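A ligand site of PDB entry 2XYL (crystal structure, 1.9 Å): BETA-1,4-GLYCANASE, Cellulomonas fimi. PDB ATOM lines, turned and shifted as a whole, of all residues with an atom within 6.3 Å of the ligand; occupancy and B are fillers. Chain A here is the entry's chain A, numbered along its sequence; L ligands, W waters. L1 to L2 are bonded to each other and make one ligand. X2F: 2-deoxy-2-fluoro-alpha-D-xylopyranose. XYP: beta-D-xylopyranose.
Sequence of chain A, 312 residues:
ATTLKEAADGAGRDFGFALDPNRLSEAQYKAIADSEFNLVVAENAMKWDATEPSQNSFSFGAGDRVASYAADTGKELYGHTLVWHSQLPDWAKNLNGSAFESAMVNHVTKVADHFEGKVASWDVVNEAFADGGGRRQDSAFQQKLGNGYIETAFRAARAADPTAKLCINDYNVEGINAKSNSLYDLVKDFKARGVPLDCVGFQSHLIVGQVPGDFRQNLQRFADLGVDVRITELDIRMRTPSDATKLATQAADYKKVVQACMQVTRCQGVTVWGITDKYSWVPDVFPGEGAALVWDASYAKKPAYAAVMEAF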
ATOM      1  N   GLU A  43      -1.229 -12.490  -3.108  1.00  0.00           N
ATOM      2  CA  GLU A  43      -2.464 -12.383  -3.872  1.00  0.00           C
ATOM      3  C   GLU A  43      -2.663 -10.939  -4.340  1.00  0.00           C
ATOM      4  O   GLU A  43      -3.104 -10.704  -5.471  1.00  0.00           O
ATOM      5  CB  GLU A  43      -3.677 -12.828  -3.038  1.00  0.00           C
ATOM      6  CG  GLU A  43      -4.997 -12.797  -3.810  1.00  0.00           C
ATOM      7  CD  GLU A  43      -6.219 -13.114  -2.949  1.00  0.00           C
ATOM      8  OE1 GLU A  43      -6.208 -12.810  -1.733  1.00  0.00           O
ATOM      9  OE2 GLU A  43      -7.211 -13.644  -3.501  1.00  0.00           O
ATOM     10  N   ASN A  44      -2.300  -9.986  -3.493  1.00  0.00           N
ATOM     11  CA  ASN A  44      -2.458  -8.569  -3.821  1.00  0.00           C
ATOM     12  C   ASN A  44      -1.362  -7.675  -3.266  1.00  0.00           C
ATOM     13  O   ASN A  44      -1.122  -6.592  -3.793  1.00  0.00           O
ATOM     14  CB  ASN A  44      -3.810  -8.044  -3.301  1.00  0.00           C
ATOM     15  CG  ASN A  44      -4.992  -8.651  -4.025  1.00  0.00           C
ATOM     16  OD1 ASN A  44      -5.273  -8.324  -5.179  1.00  0.00           O
ATOM     17  ND2 ASN A  44      -5.708  -9.536  -3.349  1.00  0.00           N
ATOM     18  N   LYS A  47       1.284  -5.877  -5.769  1.00  0.00           N
ATOM     19  CA  LYS A  47       0.811  -5.177  -6.960  1.00  0.00           C
ATOM     20  C   LYS A  47       1.127  -3.681  -6.897  1.00  0.00           C
ATOM     21  O   LYS A  47       1.556  -3.169  -5.856  1.00  0.00           O
ATOM     22  CB  LYS A  47      -0.692  -5.417  -7.170  1.00  0.00           C
ATOM     23  CG  LYS A  47      -1.022  -6.859  -7.513  1.00  0.00           C
ATOM     24  CD  LYS A  47      -2.513  -7.136  -7.536  1.00  0.00           C
ATOM     25  CE  LYS A  47      -2.773  -8.596  -7.862  1.00  0.00           C
ATOM     26  NZ  LYS A  47      -4.204  -8.977  -7.703  1.00  0.00           N
ATOM     27  N   HIS A  80       4.555 -11.319  -7.656  1.00  0.00           N
ATOM     28  CA  HIS A  80       3.428 -11.115  -8.545  1.00  0.00           C
ATOM     29  C   HIS A  80       3.240  -9.718  -9.125  1.00  0.00           C
ATOM     30  O   HIS A  80       2.915  -8.760  -8.433  1.00  0.00           O
ATOM     31  CB  HIS A  80       2.122 -11.611  -7.934  1.00  0.00           C
ATOM     32  CG  HIS A  80       0.969 -11.588  -8.888  1.00  0.00           C
ATOM     33  ND1 HIS A  80       1.081 -12.031 -10.187  1.00  0.00           N
ATOM     34  CD2 HIS A  80      -0.297 -11.132  -8.754  1.00  0.00           C
ATOM     35  CE1 HIS A  80      -0.074 -11.856 -10.810  1.00  0.00           C
ATOM     36  NE2 HIS A  80      -0.928 -11.315  -9.964  1.00  0.00           N
ATOM     37  N   THR A  81       3.443  -9.698 -10.433  1.00  0.00           N
ATOM     38  CA  THR A  81       3.346  -8.549 -11.322  1.00  0.00           C
ATOM     39  C   THR A  81       3.808  -7.133 -10.982  1.00  0.00           C
ATOM     40  O   THR A  81       3.304  -6.476 -10.064  1.00  0.00           O
ATOM     41  CB  THR A  81       1.985  -8.518 -12.027  1.00  0.00           C
ATOM     42  OG1 THR A  81       2.107  -7.793 -13.252  1.00  0.00           O
ATOM     43  CG2 THR A  81       0.916  -7.879 -11.147  1.00  0.00           C
ATOM     44  N   TRP A  84       0.972  -4.173 -14.906  1.00  0.00           N
ATOM     45  CA  TRP A  84      -0.359  -4.726 -15.144  1.00  0.00           C
ATOM     46  C   TRP A  84      -1.354  -3.587 -15.315  1.00  0.00           C
ATOM     47  O   TRP A  84      -1.339  -2.627 -14.544  1.00  0.00           O
ATOM     48  CB  TRP A  84      -0.761  -5.602 -13.956  1.00  0.00           C
ATOM     49  CG  TRP A  84      -1.990  -6.423 -14.168  1.00  0.00           C
ATOM     50  CD1 TRP A  84      -2.454  -6.916 -15.351  1.00  0.00           C
ATOM     51  CD2 TRP A  84      -2.896  -6.897 -13.161  1.00  0.00           C
ATOM     52  NE1 TRP A  84      -3.596  -7.651 -15.143  1.00  0.00           N
ATOM     53  CE2 TRP A  84      -3.891  -7.659 -13.808  1.00  0.00           C
ATOM     54  CE3 TRP A  84      -2.963  -6.736 -11.766  1.00  0.00           C
ATOM     55  CZ2 TRP A  84      -4.941  -8.271 -13.117  1.00  0.00           C
ATOM     56  CZ3 TRP A  84      -4.007  -7.342 -11.081  1.00  0.00           C
ATOM     57  CH2 TRP A  84      -4.985  -8.095 -11.755  1.00  0.00           C
ATOM     58  N   SER A  86      -4.539  -3.644 -14.763  1.00  0.00           N
ATOM     59  CA  SER A  86      -5.522  -3.631 -13.675  1.00  0.00           C
ATOM     60  C   SER A  86      -4.847  -3.284 -12.347  1.00  0.00           C
ATOM     61  O   SER A  86      -3.648  -3.486 -12.177  1.00  0.00           O
ATOM     62  CB  SER A  86      -6.233  -4.986 -13.585  1.00  0.00           C
ATOM     63  OG  SER A  86      -7.316  -4.941 -12.671  1.00  0.00           O
ATOM     64  N   GLN A  87      -5.644  -2.766 -11.412  1.00  0.00           N
ATOM     65  CA  GLN A  87      -5.160  -2.352 -10.098  1.00  0.00           C
ATOM     66  C   GLN A  87      -3.982  -1.386 -10.211  1.00  0.00           C
ATOM     67  O   GLN A  87      -2.948  -1.558  -9.563  1.00  0.00           O
ATOM     68  CB  GLN A  87      -4.825  -3.564  -9.217  1.00  0.00           C
ATOM     69  CG  GLN A  87      -6.059  -4.246  -8.665  1.00  0.00           C
ATOM     70  CD  GLN A  87      -5.725  -5.378  -7.713  1.00  0.00           C
ATOM     71  OE1 GLN A  87      -5.441  -5.150  -6.539  1.00  0.00           O
ATOM     72  NE2 GLN A  87      -5.787  -6.604  -8.213  1.00  0.00           N
ATOM     73  N   ASP A 123       6.565 -11.747 -12.223  1.00  0.00           N
ATOM     74  CA  ASP A 123       5.607 -11.634 -13.314  1.00  0.00           C
ATOM     75  C   ASP A 123       5.887 -10.202 -13.738  1.00  0.00           C
ATOM     76  O   ASP A 123       5.320  -9.271 -13.178  1.00  0.00           O
ATOM     77  CB  ASP A 123       4.161 -11.760 -12.814  1.00  0.00           C
ATOM     78  CG  ASP A 123       3.660 -13.181 -12.785  1.00  0.00           C
ATOM     79  OD1 ASP A 123       4.237 -14.053 -13.467  1.00  0.00           O
ATOM     80  OD2 ASP A 123       2.656 -13.436 -12.085  1.00  0.00           O
ATOM     81  N   ASN A 126       1.959  -8.741 -16.986  1.00  0.00           N
ATOM     82  CA  ASN A 126       0.802  -9.597 -16.801  1.00  0.00           C
ATOM     83  C   ASN A 126      -0.358  -9.156 -17.697  1.00  0.00           C
ATOM     84  O   ASN A 126      -0.673  -7.964 -17.783  1.00  0.00           O
ATOM     85  CB  ASN A 126       0.367  -9.548 -15.328  1.00  0.00           C
ATOM     86  CG  ASN A 126      -0.729 -10.536 -14.993  1.00  0.00           C
ATOM     87  OD1 ASN A 126      -0.577 -11.741 -15.213  1.00  0.00           O
ATOM     88  ND2 ASN A 126      -1.809 -10.043 -14.412  1.00  0.00           N
ATOM     89  N   GLU A 127      -0.934 -10.116 -18.426  1.00  0.00           N
ATOM     90  CA  GLU A 127      -2.079  -9.888 -19.307  1.00  0.00           C
ATOM     91  C   GLU A 127      -1.917  -8.766 -20.341  1.00  0.00           C
ATOM     92  O   GLU A 127      -2.729  -7.836 -20.395  1.00  0.00           O
ATOM     93  CB  GLU A 127      -3.327  -9.664 -18.454  1.00  0.00           C
ATOM     94  CG  GLU A 127      -3.575 -10.808 -17.479  1.00  0.00           C
ATOM     95  CD  GLU A 127      -4.673 -10.528 -16.482  1.00  0.00           C
ATOM     96  OE1 GLU A 127      -5.401  -9.516 -16.630  1.00  0.00           O
ATOM     97  OE2 GLU A 127      -4.812 -11.330 -15.541  1.00  0.00           O
ATOM     98  N   ASN A 169       3.076 -13.297 -17.868  1.00  0.00           N
ATOM     99  CA  ASN A 169       1.907 -14.062 -17.431  1.00  0.00           C
ATOM    100  C   ASN A 169       0.634 -13.700 -18.188  1.00  0.00           C
ATOM    101  O   ASN A 169       0.457 -12.556 -18.603  1.00  0.00           O
ATOM    102  CB  ASN A 169       1.724 -13.829 -15.932  1.00  0.00           C
ATOM    103  CG  ASN A 169       0.855 -14.878 -15.270  1.00  0.00           C
ATOM    104  OD1 ASN A 169       1.018 -16.071 -15.501  1.00  0.00           O
ATOM    105  ND2 ASN A 169      -0.079 -14.435 -14.431  1.00  0.00           N
ATOM    106  N   GLN A 203      -2.018 -18.751 -16.381  1.00  0.00           N
ATOM    107  CA  GLN A 203      -2.959 -18.563 -15.290  1.00  0.00           C
ATOM    108  C   GLN A 203      -3.803 -19.786 -14.958  1.00  0.00           C
ATOM    109  O   GLN A 203      -3.855 -20.223 -13.812  1.00  0.00           O
ATOM    110  CB  GLN A 203      -3.835 -17.335 -15.531  1.00  0.00           C
ATOM    111  CG  GLN A 203      -3.042 -16.034 -15.504  1.00  0.00           C
ATOM    112  CD  GLN A 203      -3.905 -14.790 -15.444  1.00  0.00           C
ATOM    113  OE1 GLN A 203      -5.081 -14.847 -15.117  1.00  0.00           O
ATOM    114  NE2 GLN A 203      -3.302 -13.653 -15.757  1.00  0.00           N
ATOM    115  N   HIS A 205      -7.244 -20.245 -15.220  1.00  0.00           N
ATOM    116  CA  HIS A 205      -8.516 -19.967 -14.549  1.00  0.00           C
ATOM    117  C   HIS A 205      -9.535 -20.703 -15.411  1.00  0.00           C
ATOM    118  O   HIS A 205     -10.189 -20.117 -16.280  1.00  0.00           O
ATOM    119  CB  HIS A 205      -8.812 -18.464 -14.508  1.00  0.00           C
ATOM    120  CG  HIS A 205      -8.001 -17.714 -13.499  1.00  0.00           C
ATOM    121  ND1 HIS A 205      -8.067 -17.967 -12.147  1.00  0.00           N
ATOM    122  CD2 HIS A 205      -7.100 -16.702 -13.647  1.00  0.00           C
ATOM    123  CE1 HIS A 205      -7.247 -17.144 -11.501  1.00  0.00           C
ATOM    124  NE2 HIS A 205      -6.651 -16.374 -12.390  1.00  0.00           N
ATOM    125  N   GLU A 233      -2.071 -19.352 -11.676  1.00  0.00           N
ATOM    126  CA  GLU A 233      -3.234 -19.025 -10.857  1.00  0.00           C
ATOM    127  C   GLU A 233      -4.373 -20.006 -11.009  1.00  0.00           C
ATOM    128  O   GLU A 233      -5.524 -19.619 -11.232  1.00  0.00           O
ATOM    129  CB  GLU A 233      -3.692 -17.617 -11.230  1.00  0.00           C
ATOM    130  CG  GLU A 233      -2.572 -16.621 -11.370  1.00  0.00           C
ATOM    131  CD  GLU A 233      -3.047 -15.257 -11.846  1.00  0.00           C
ATOM    132  OE1 GLU A 233      -4.266 -14.712 -11.314  1.00  0.00           O
ATOM    133  OE2 GLU A 233      -2.350 -14.661 -12.680  1.00  0.00           O
ATOM    134  N   TRP A 273      -4.668 -20.460  -6.967  1.00  0.00           N
ATOM    135  CA  TRP A 273      -5.012 -19.123  -6.525  1.00  0.00           C
ATOM    136  C   TRP A 273      -5.828 -19.076  -5.227  1.00  0.00           C
ATOM    137  O   TRP A 273      -6.984 -18.652  -5.216  1.00  0.00           O
ATOM    138  CB  TRP A 273      -5.688 -18.331  -7.640  1.00  0.00           C
ATOM    139  CG  TRP A 273      -5.423 -16.862  -7.534  1.00  0.00           C
ATOM    140  CD1 TRP A 273      -6.357 -15.877  -7.362  1.00  0.00           C
ATOM    141  CD2 TRP A 273      -4.152 -16.224  -7.536  1.00  0.00           C
ATOM    142  NE1 TRP A 273      -5.730 -14.653  -7.247  1.00  0.00           N
ATOM    143  CE2 TRP A 273      -4.376 -14.842  -7.356  1.00  0.00           C
ATOM    144  CE3 TRP A 273      -2.834 -16.680  -7.670  1.00  0.00           C
ATOM    145  CZ2 TRP A 273      -3.329 -13.913  -7.301  1.00  0.00           C
ATOM    146  CZ3 TRP A 273      -1.793 -15.753  -7.623  1.00  0.00           C
ATOM    147  CH2 TRP A 273      -2.051 -14.385  -7.440  1.00  0.00           C
ATOM    148  N   TRP A 281     -11.543 -15.658  -4.968  1.00  0.00           N
ATOM    149  CA  TRP A 281     -11.958 -14.445  -5.678  1.00  0.00           C
ATOM    150  C   TRP A 281     -13.050 -14.686  -6.716  1.00  0.00           C
ATOM    151  O   TRP A 281     -13.719 -13.744  -7.153  1.00  0.00           O
ATOM    152  CB  TRP A 281     -10.747 -13.811  -6.378  1.00  0.00           C
ATOM    153  CG  TRP A 281     -10.342 -14.528  -7.662  1.00  0.00           C
ATOM    154  CD1 TRP A 281     -10.072 -15.860  -7.812  1.00  0.00           C
ATOM    155  CD2 TRP A 281     -10.206 -13.937  -8.967  1.00  0.00           C
ATOM    156  NE1 TRP A 281      -9.784 -16.137  -9.126  1.00  0.00           N
ATOM    157  CE2 TRP A 281      -9.852 -14.980  -9.850  1.00  0.00           C
ATOM    158  CE3 TRP A 281     -10.340 -12.643  -9.461  1.00  0.00           C
ATOM    159  CZ2 TRP A 281      -9.641 -14.755 -11.212  1.00  0.00           C
ATOM    160  CZ3 TRP A 281     -10.129 -12.418 -10.823  1.00  0.00           C
ATOM    161  CH2 TRP A 281      -9.786 -13.477 -11.681  1.00  0.00           C
ATOM    162  N   VAL A 285     -16.104 -12.091  -9.026  1.00  0.00           N
ATOM    163  CA  VAL A 285     -15.843 -11.778 -10.420  1.00  0.00           C
ATOM    164  C   VAL A 285     -16.787 -12.536 -11.357  1.00  0.00           C
ATOM    165  O   VAL A 285     -17.302 -11.973 -12.308  1.00  0.00           O
ATOM    166  CB  VAL A 285     -14.372 -12.116 -10.793  1.00  0.00           C
ATOM    167  CG1 VAL A 285     -14.116 -11.886 -12.265  1.00  0.00           C
ATOM    168  CG2 VAL A 285     -13.419 -11.279  -9.958  1.00  0.00           C
HETATM  169  C1  X2F L   1      -4.859 -13.649 -12.062  1.00  0.00           C
HETATM  170  C2  X2F L   1      -4.205 -12.277 -11.737  1.00  0.00           C
HETATM  171  C3  X2F L   1      -4.326 -11.929 -10.246  1.00  0.00           C
HETATM  172  C4  X2F L   1      -5.796 -11.967  -9.874  1.00  0.00           C
HETATM  173  C5  X2F L   1      -6.376 -13.315 -10.296  1.00  0.00           C
HETATM  174  O3  X2F L   1      -3.810 -10.630  -9.980  1.00  0.00           O
HETATM  175  O4  X2F L   1      -5.944 -11.823  -8.455  1.00  0.00           O
HETATM  176  O5  X2F L   1      -6.228 -13.487 -11.709  1.00  0.00           O
HETATM  177  F2  X2F L   1      -2.897 -12.200 -12.214  1.00  0.00           F
HETATM  178  C1  XYP L   2      -7.063 -11.109  -8.048  1.00  0.00           C
HETATM  179  C2  XYP L   2      -7.205 -11.227  -6.534  1.00  0.00           C
HETATM  180  C3  XYP L   2      -8.332 -10.371  -5.978  1.00  0.00           C
HETATM  181  C4  XYP L   2      -8.167  -8.950  -6.479  1.00  0.00           C
HETATM  182  C5  XYP L   2      -8.098  -8.928  -7.993  1.00  0.00           C
HETATM  183  O2  XYP L   2      -7.395 -12.565  -6.185  1.00  0.00           O
HETATM  184  O3  XYP L   2      -8.257 -10.392  -4.569  1.00  0.00           O
HETATM  185  O4  XYP L   2      -9.264  -8.159  -6.055  1.00  0.00           O
HETATM  186  O5  XYP L   2      -6.994  -9.746  -8.440  1.00  0.00           O
HETATM  187  O   HOH W   1     -10.935 -11.358  -3.908  1.00  0.00           O
HETATM  188  O   HOH W   2      -7.654  -6.615 -10.350  1.00  0.00           O
HETATM  189  O   HOH W   3     -11.774  -9.230  -7.328  1.00  0.00           O
HETATM  190  O   HOH W   4      -7.065 -11.232 -13.702  1.00  0.00           O
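An oxygen (O5) of X2F L1 lies within hydrogen-bond range of a ring nitrogen (NE2) of His 205, 3.0 Å away.
NE2 of Gln 87 lies close to O5 of XYP L2, 3.4 Å away.
NE2 of His 80 sits at hydrogen-bond distance from O3 of X2F L1.
The side-chain carboxylate (OE2) of Glu 43 is in hydrogen-bond range of an oxygen (O2) of XYP L2, at 2.9 Å.
NE1 of Trp 273 lies within hydrogen-bond range of O2 of XYP L2 (2.9 Å).
An oxygen (O3) of X2F L1 is in hydrogen-bond range of the side-chain amino group (NZ) of Lys 47.
An oxygen (O3) of XYP L2 sits at hydrogen-bond distance from the side-chain amide nitrogen (ND2) of Asn 44 (3.0 Å).
The side-chain carboxylate (OE1) of Glu 233 is covalently linked to a carbon (C1) of X2F L1 (1.4 Å).
The indole nitrogen (NE1) of Trp 84 lies within hydrogen-bond range of the side-chain carboxylate (OE1) of Glu 127.
OE1 of Gln 87 sits close to OD1 of Asn 44 (3.5 Å).
ND2 of Asn 169 sits at hydrogen-bond distance from OE2 of Glu 233 (2.9 Å).
The backbone NH (N) of Glu 127 lies within hydrogen-bond range of the backbone carbonyl oxygen (O) of Asn 169, 2.8 Å away.
NZ of Lys 47 sits close to NE2 of Gln 87, at 2.9 Å.
OD1 of Asn 44 lies within hydrogen-bond range of NZ of Lys 47, at 2.8 Å.
ND2 of Asn 126 lies within hydrogen-bond range of OE2 of Glu 127 (3.5 Å).
NE2 of His 205 sits close to OE1 of Gln 203 (3.5 Å).
The side-chain amide nitrogen (ND2) of Asn 126 sits close to a fluorine (F2) of X2F L1, 3.3 Å away.
Trp 84 touches the ligand.
OE2 of Glu 127 touches F2 of X2F L1, at 3.9 Å.
OE1 of Gln 203 touches C1 of X2F L1 (3.3 Å).
Trp 281 touches the ligand.
Hydrophobic or aromatic side chains that line the ligand: His 80, Trp 84, His 205, Trp 273 and Trp 281.
Of the 18 residues printed, 13 come within 4 Å of the ligand.
The nearest printed residue that does not touch the ligand is Asn 169 (4.2 Å).
Water W4 lies within hydrogen-bond range of OE2 of Glu 127 and O5 of X2F L1.
Water W2 lies within hydrogen-bond range of the side-chain amide nitrogen of Gln 87 (2.8 Å) and the side-chain hydroxyl of Ser 86 (2.9 Å).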
